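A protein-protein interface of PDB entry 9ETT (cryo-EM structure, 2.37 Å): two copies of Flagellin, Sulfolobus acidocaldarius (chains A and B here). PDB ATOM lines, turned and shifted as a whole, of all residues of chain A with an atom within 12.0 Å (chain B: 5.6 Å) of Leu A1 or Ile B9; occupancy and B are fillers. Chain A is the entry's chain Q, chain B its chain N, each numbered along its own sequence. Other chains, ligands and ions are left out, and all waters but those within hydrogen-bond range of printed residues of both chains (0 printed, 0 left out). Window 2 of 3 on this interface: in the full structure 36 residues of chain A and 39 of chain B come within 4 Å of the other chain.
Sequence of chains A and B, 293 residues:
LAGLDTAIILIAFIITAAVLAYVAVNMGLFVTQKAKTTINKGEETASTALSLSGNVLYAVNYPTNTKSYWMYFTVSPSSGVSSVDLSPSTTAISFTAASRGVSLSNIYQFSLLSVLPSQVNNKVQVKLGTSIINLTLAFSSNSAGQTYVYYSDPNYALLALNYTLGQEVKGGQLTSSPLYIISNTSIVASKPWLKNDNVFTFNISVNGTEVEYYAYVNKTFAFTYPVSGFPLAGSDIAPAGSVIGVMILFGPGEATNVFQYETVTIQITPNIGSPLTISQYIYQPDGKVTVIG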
ATOM      1  N   LEU A   1      -2.816 -10.870  -6.964  1.00  0.00           N
ATOM      2  CA  LEU A   1      -2.202 -10.433  -5.680  1.00  0.00           C
ATOM      3  C   LEU A   1      -1.771  -8.970  -5.791  1.00  0.00           C
ATOM      4  O   LEU A   1      -2.004  -8.196  -4.865  1.00  0.00           O
ATOM      5  CB  LEU A   1      -1.033 -11.360  -5.324  1.00  0.00           C
ATOM      6  CG  LEU A   1       0.131 -10.767  -4.524  1.00  0.00           C
ATOM      7  CD1 LEU A   1      -0.303 -10.121  -3.209  1.00  0.00           C
ATOM      8  CD2 LEU A   1       1.183 -11.831  -4.289  1.00  0.00           C
ATOM      9  N   ALA A   2      -1.166  -8.583  -6.923  1.00  0.00           N
ATOM     10  CA  ALA A   2      -0.595  -7.249  -7.031  1.00  0.00           C
ATOM     11  C   ALA A   2      -1.621  -6.197  -6.617  1.00  0.00           C
ATOM     12  O   ALA A   2      -1.234  -5.241  -5.959  1.00  0.00           O
ATOM     13  CB  ALA A   2      -0.021  -6.993  -8.393  1.00  0.00           C
ATOM     14  N   GLY A   3      -2.916  -6.430  -6.896  1.00  0.00           N
ATOM     15  CA  GLY A   3      -4.000  -5.520  -6.543  1.00  0.00           C
ATOM     16  C   GLY A   3      -4.554  -5.742  -5.133  1.00  0.00           C
ATOM     17  O   GLY A   3      -4.887  -4.774  -4.455  1.00  0.00           O
ATOM     18  N   LEU A   4      -4.656  -7.006  -4.697  1.00  0.00           N
ATOM     19  CA  LEU A   4      -5.243  -7.339  -3.406  1.00  0.00           C
ATOM     20  C   LEU A   4      -4.506  -6.609  -2.279  1.00  0.00           C
ATOM     21  O   LEU A   4      -5.149  -5.926  -1.485  1.00  0.00           O
ATOM     22  CB  LEU A   4      -5.235  -8.861  -3.218  1.00  0.00           C
ATOM     23  CG  LEU A   4      -6.497  -9.496  -2.631  1.00  0.00           C
ATOM     24  CD1 LEU A   4      -7.769  -8.944  -3.265  1.00  0.00           C
ATOM     25  CD2 LEU A   4      -6.451 -10.997  -2.860  1.00  0.00           C
ATOM     26  N   ASP A   5      -3.169  -6.734  -2.239  1.00  0.00           N
ATOM     27  CA  ASP A   5      -2.339  -6.045  -1.257  1.00  0.00           C
ATOM     28  C   ASP A   5      -2.372  -4.535  -1.512  1.00  0.00           C
ATOM     29  O   ASP A   5      -2.377  -3.745  -0.570  1.00  0.00           O
ATOM     30  CB  ASP A   5      -0.908  -6.595  -1.230  1.00  0.00           C
ATOM     31  CG  ASP A   5       0.090  -5.649  -1.871  1.00  0.00           C
ATOM     32  OD1 ASP A   5       0.200  -5.659  -3.117  1.00  0.00           O
ATOM     33  OD2 ASP A   5       0.720  -4.885  -1.117  1.00  0.00           O
ATOM     34  N   THR A   6      -2.393  -4.141  -2.794  1.00  0.00           N
ATOM     35  CA  THR A   6      -2.451  -2.744  -3.207  1.00  0.00           C
ATOM     36  C   THR A   6      -3.787  -2.129  -2.779  1.00  0.00           C
ATOM     37  O   THR A   6      -3.860  -0.922  -2.572  1.00  0.00           O
ATOM     38  CB  THR A   6      -2.210  -2.622  -4.720  1.00  0.00           C
ATOM     39  OG1 THR A   6      -0.807  -2.706  -4.953  1.00  0.00           O
ATOM     40  CG2 THR A   6      -2.722  -1.342  -5.337  1.00  0.00           C
ATOM     41  N   ALA A   7      -4.834  -2.962  -2.656  1.00  0.00           N
ATOM     42  CA  ALA A   7      -6.161  -2.538  -2.226  1.00  0.00           C
ATOM     43  C   ALA A   7      -6.195  -2.332  -0.710  1.00  0.00           C
ATOM     44  O   ALA A   7      -7.050  -1.606  -0.211  1.00  0.00           O
ATOM     45  CB  ALA A   7      -7.194  -3.544  -2.672  1.00  0.00           C
ATOM     46  N   ILE A   8      -5.277  -2.989   0.019  1.00  0.00           N
ATOM     47  CA  ILE A   8      -5.147  -2.842   1.465  1.00  0.00           C
ATOM     48  C   ILE A   8      -4.517  -1.488   1.795  1.00  0.00           C
ATOM     49  O   ILE A   8      -4.870  -0.882   2.801  1.00  0.00           O
ATOM     50  CB  ILE A   8      -4.329  -4.001   2.075  1.00  0.00           C
ATOM     51  CG1 ILE A   8      -5.064  -5.340   1.985  1.00  0.00           C
ATOM     52  CG2 ILE A   8      -3.895  -3.686   3.503  1.00  0.00           C
ATOM     53  CD1 ILE A   8      -4.162  -6.531   2.183  1.00  0.00           C
ATOM     54  N   ILE A   9      -3.583  -1.020   0.953  1.00  0.00           N
ATOM     55  CA  ILE A   9      -2.858   0.233   1.166  1.00  0.00           C
ATOM     56  C   ILE A   9      -3.717   1.431   0.758  1.00  0.00           C
ATOM     57  O   ILE A   9      -3.495   2.530   1.257  1.00  0.00           O
ATOM     58  CB  ILE A   9      -1.497   0.223   0.436  1.00  0.00           C
ATOM     59  CG1 ILE A   9      -0.612  -0.926   0.925  1.00  0.00           C
ATOM     60  CG2 ILE A   9      -0.787   1.572   0.564  1.00  0.00           C
ATOM     61  CD1 ILE A   9       0.019  -1.723  -0.184  1.00  0.00           C
ATOM     62  N   LEU A  10      -4.639   1.229  -0.194  1.00  0.00           N
ATOM     63  CA  LEU A  10      -5.589   2.254  -0.603  1.00  0.00           C
ATOM     64  C   LEU A  10      -6.640   2.496   0.488  1.00  0.00           C
ATOM     65  O   LEU A  10      -6.781   3.633   0.920  1.00  0.00           O
ATOM     66  CB  LEU A  10      -6.176   1.887  -1.971  1.00  0.00           C
ATOM     67  CG  LEU A  10      -7.351   2.723  -2.474  1.00  0.00           C
ATOM     68  CD1 LEU A  10      -7.003   4.201  -2.548  1.00  0.00           C
ATOM     69  CD2 LEU A  10      -7.799   2.219  -3.832  1.00  0.00           C
ATOM     70  N   ILE A  11      -7.315   1.445   0.983  1.00  0.00           N
ATOM     71  CA  ILE A  11      -8.255   1.540   2.098  1.00  0.00           C
ATOM     72  C   ILE A  11      -7.641   2.302   3.281  1.00  0.00           C
ATOM     73  O   ILE A  11      -8.204   3.290   3.756  1.00  0.00           O
ATOM     74  CB  ILE A  11      -8.788   0.138   2.475  1.00  0.00           C
ATOM     75  CG1 ILE A  11      -9.742  -0.390   1.401  1.00  0.00           C
ATOM     76  CG2 ILE A  11      -9.444   0.106   3.856  1.00  0.00           C
ATOM     77  CD1 ILE A  11      -9.955  -1.892   1.423  1.00  0.00           C
ATOM     78  N   ASP B   5       2.141 -22.501  -4.164  1.00  0.00           N
ATOM     79  CA  ASP B   5       3.248 -21.605  -3.843  1.00  0.00           C
ATOM     80  C   ASP B   5       2.817 -20.149  -4.051  1.00  0.00           C
ATOM     81  O   ASP B   5       3.210 -19.268  -3.287  1.00  0.00           O
ATOM     82  CB  ASP B   5       4.513 -21.950  -4.637  1.00  0.00           C
ATOM     83  CG  ASP B   5       4.795 -20.954  -5.746  1.00  0.00           C
ATOM     84  OD1 ASP B   5       4.184 -21.084  -6.828  1.00  0.00           O
ATOM     85  OD2 ASP B   5       5.597 -20.033  -5.500  1.00  0.00           O
ATOM     86  N   THR B   6       2.010 -19.903  -5.092  1.00  0.00           N
ATOM     87  CA  THR B   6       1.491 -18.579  -5.412  1.00  0.00           C
ATOM     88  C   THR B   6       0.546 -18.107  -4.301  1.00  0.00           C
ATOM     89  O   THR B   6       0.395 -16.906  -4.104  1.00  0.00           O
ATOM     90  CB  THR B   6       0.812 -18.587  -6.791  1.00  0.00           C
ATOM     91  OG1 THR B   6       1.832 -18.506  -7.785  1.00  0.00           O
ATOM     92  CG2 THR B   6      -0.171 -17.463  -7.015  1.00  0.00           C
ATOM     93  N   ALA B   7      -0.088 -19.055  -3.591  1.00  0.00           N
ATOM     94  CA  ALA B   7      -0.989 -18.770  -2.480  1.00  0.00           C
ATOM     95  C   ALA B   7      -0.195 -18.407  -1.223  1.00  0.00           C
ATOM     96  O   ALA B   7      -0.732 -17.756  -0.333  1.00  0.00           O
ATOM     97  CB  ALA B   7      -1.899 -19.950  -2.237  1.00  0.00           C
ATOM     98  N   ILE B   8       1.071 -18.851  -1.147  1.00  0.00           N
ATOM     99  CA  ILE B   8       1.967 -18.534  -0.040  1.00  0.00           C
ATOM    100  C   ILE B   8       2.426 -17.078  -0.148  1.00  0.00           C
ATOM    101  O   ILE B   8       2.603 -16.420   0.872  1.00  0.00           O
ATOM    102  CB  ILE B   8       3.173 -19.498   0.002  1.00  0.00           C
ATOM    103  CG1 ILE B   8       2.760 -20.926   0.364  1.00  0.00           C
ATOM    104  CG2 ILE B   8       4.274 -18.974   0.918  1.00  0.00           C
ATOM    105  CD1 ILE B   8       3.806 -21.957   0.024  1.00  0.00           C
ATOM    106  N   ILE B   9       2.624 -16.582  -1.378  1.00  0.00           N
ATOM    107  CA  ILE B   9       3.111 -15.228  -1.634  1.00  0.00           C
ATOM    108  C   ILE B   9       1.980 -14.207  -1.487  1.00  0.00           C
ATOM    109  O   ILE B   9       2.253 -13.040  -1.216  1.00  0.00           O
ATOM    110  CB  ILE B   9       3.800 -15.130  -3.016  1.00  0.00           C
ATOM    111  CG1 ILE B   9       4.988 -16.090  -3.112  1.00  0.00           C
ATOM    112  CG2 ILE B   9       4.214 -13.691  -3.330  1.00  0.00           C
ATOM    113  CD1 ILE B   9       5.012 -16.910  -4.373  1.00  0.00           C
ATOM    114  N   LEU B  10       0.735 -14.634  -1.735  1.00  0.00           N
ATOM    115  CA  LEU B  10      -0.441 -13.799  -1.536  1.00  0.00           C
ATOM    116  C   LEU B  10      -0.716 -13.584  -0.042  1.00  0.00           C
ATOM    117  O   LEU B  10      -0.783 -12.435   0.381  1.00  0.00           O
ATOM    118  CB  LEU B  10      -1.624 -14.388  -2.314  1.00  0.00           C
ATOM    119  CG  LEU B  10      -3.002 -13.782  -2.051  1.00  0.00           C
ATOM    120  CD1 LEU B  10      -3.027 -12.290  -2.336  1.00  0.00           C
ATOM    121  CD2 LEU B  10      -4.051 -14.497  -2.882  1.00  0.00           C
ATOM    122  N   ILE B  11      -0.799 -14.657   0.763  1.00  0.00           N
ATOM    123  CA  ILE B  11      -0.949 -14.571   2.216  1.00  0.00           C
ATOM    124  C   ILE B  11       0.083 -13.611   2.824  1.00  0.00           C
ATOM    125  O   ILE B  11      -0.277 -12.662   3.523  1.00  0.00           O
ATOM    126  CB  ILE B  11      -0.924 -15.984   2.843  1.00  0.00           C
ATOM    127  CG1 ILE B  11      -2.209 -16.749   2.518  1.00  0.00           C
ATOM    128  CG2 ILE B  11      -0.667 -15.958   4.350  1.00  0.00           C
ATOM    129  CD1 ILE B  11      -2.109 -18.254   2.675  1.00  0.00           C
ATOM    130  N   ALA B  12       1.363 -13.816   2.501  1.00  0.00           N
ATOM    131  CA  ALA B  12       2.469 -13.033   3.039  1.00  0.00           C
ATOM    132  C   ALA B  12       2.402 -11.554   2.638  1.00  0.00           C
ATOM    133  O   ALA B  12       2.632 -10.665   3.460  1.00  0.00           O
ATOM    134  CB  ALA B  12       3.755 -13.675   2.599  1.00  0.00           C
ATOM    135  N   PHE B  13       2.096 -11.272   1.366  1.00  0.00           N
ATOM    136  CA  PHE B  13       2.019  -9.905   0.870  1.00  0.00           C
ATOM    137  C   PHE B  13       0.806  -9.165   1.438  1.00  0.00           C
ATOM    138  O   PHE B  13       0.916  -7.972   1.700  1.00  0.00           O
ATOM    139  CB  PHE B  13       2.048  -9.892  -0.660  1.00  0.00           C
ATOM    140  CG  PHE B  13       3.392 -10.115  -1.327  1.00  0.00           C
ATOM    141  CD1 PHE B  13       4.502 -10.585  -0.627  1.00  0.00           C
ATOM    142  CD2 PHE B  13       3.553  -9.851  -2.681  1.00  0.00           C
ATOM    143  CE1 PHE B  13       5.725 -10.792  -1.253  1.00  0.00           C
ATOM    144  CE2 PHE B  13       4.775 -10.049  -3.310  1.00  0.00           C
ATOM    145  CZ  PHE B  13       5.857 -10.521  -2.595  1.00  0.00           C
ATOM    146  N   ILE B  14      -0.314  -9.860   1.692  1.00  0.00           N
ATOM    147  CA  ILE B  14      -1.465  -9.287   2.389  1.00  0.00           C
ATOM    148  C   ILE B  14      -1.042  -8.827   3.782  1.00  0.00           C
ATOM    149  O   ILE B  14      -1.275  -7.680   4.142  1.00  0.00           O
ATOM    150  CB  ILE B  14      -2.650 -10.279   2.461  1.00  0.00           C
ATOM    151  CG1 ILE B  14      -3.264 -10.579   1.088  1.00  0.00           C
ATOM    152  CG2 ILE B  14      -3.703  -9.862   3.487  1.00  0.00           C
ATOM    153  CD1 ILE B  14      -4.031  -9.439   0.436  1.00  0.00           C
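Among the printed residues, pairs that only touch across the chains: Ile A8 with Ile B14, Leu A1 with Ile B9, Leu A1 with Phe B13, Leu A1 with Leu B10, Leu A4 with Leu B10, Asp A5 with Phe B13, Leu A4 with Ile B14 and Asp A5 with Ile B14.
Leu A1 touches three residues of chain B.
Ile B9 touches just one residue of chain A: Leu A1.
No residue of chain A comes within 4 Å of Asp B5.
No residue of chain A comes within 4 Å of Ala B7.
Of the printed residues of chain A, Leu B10 touches Leu A1 and Leu A4.
No residue of chain A comes within 4 Å of Ile B11.
No residue of chain A comes within 4 Å of Ala B12.
Of chain A, only Leu A1 and Asp A5 come within 4 Å of Phe B13.
Ile B14 touches three residues of chain A.
Printed residues of chain B within 4 Å of Ile A8: Ile B14.
Of the printed residues of chain B, Leu A4 touches Leu B10 (3.7 Å) and Ile B14 (3.9 Å).
Leu A10 touches none of the printed residues of chain B.
The nearest printed residue of chain B that does not touch Asp A5 is Leu B10 (5.6 Å).
Of the 11 printed residues of chain A, 4 touch a printed residue of chain B.
Printed residues of chain A that touch a printed residue of chain B: Leu A1, Leu A4, Asp A5 and Ile A8.
Hydrophobic or aromatic side chains of chain A within 4 Å of the printed part of chain B: Leu A1, Leu A4 and Ile A8.
Among the printed residues, no Asp or Glu carboxylate lies within 4 Å of a Lys or Arg side-chain nitrogen of the other chain.
Positions printed for both chains: 5, 6, 7, 8, 9, 10 and 11.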
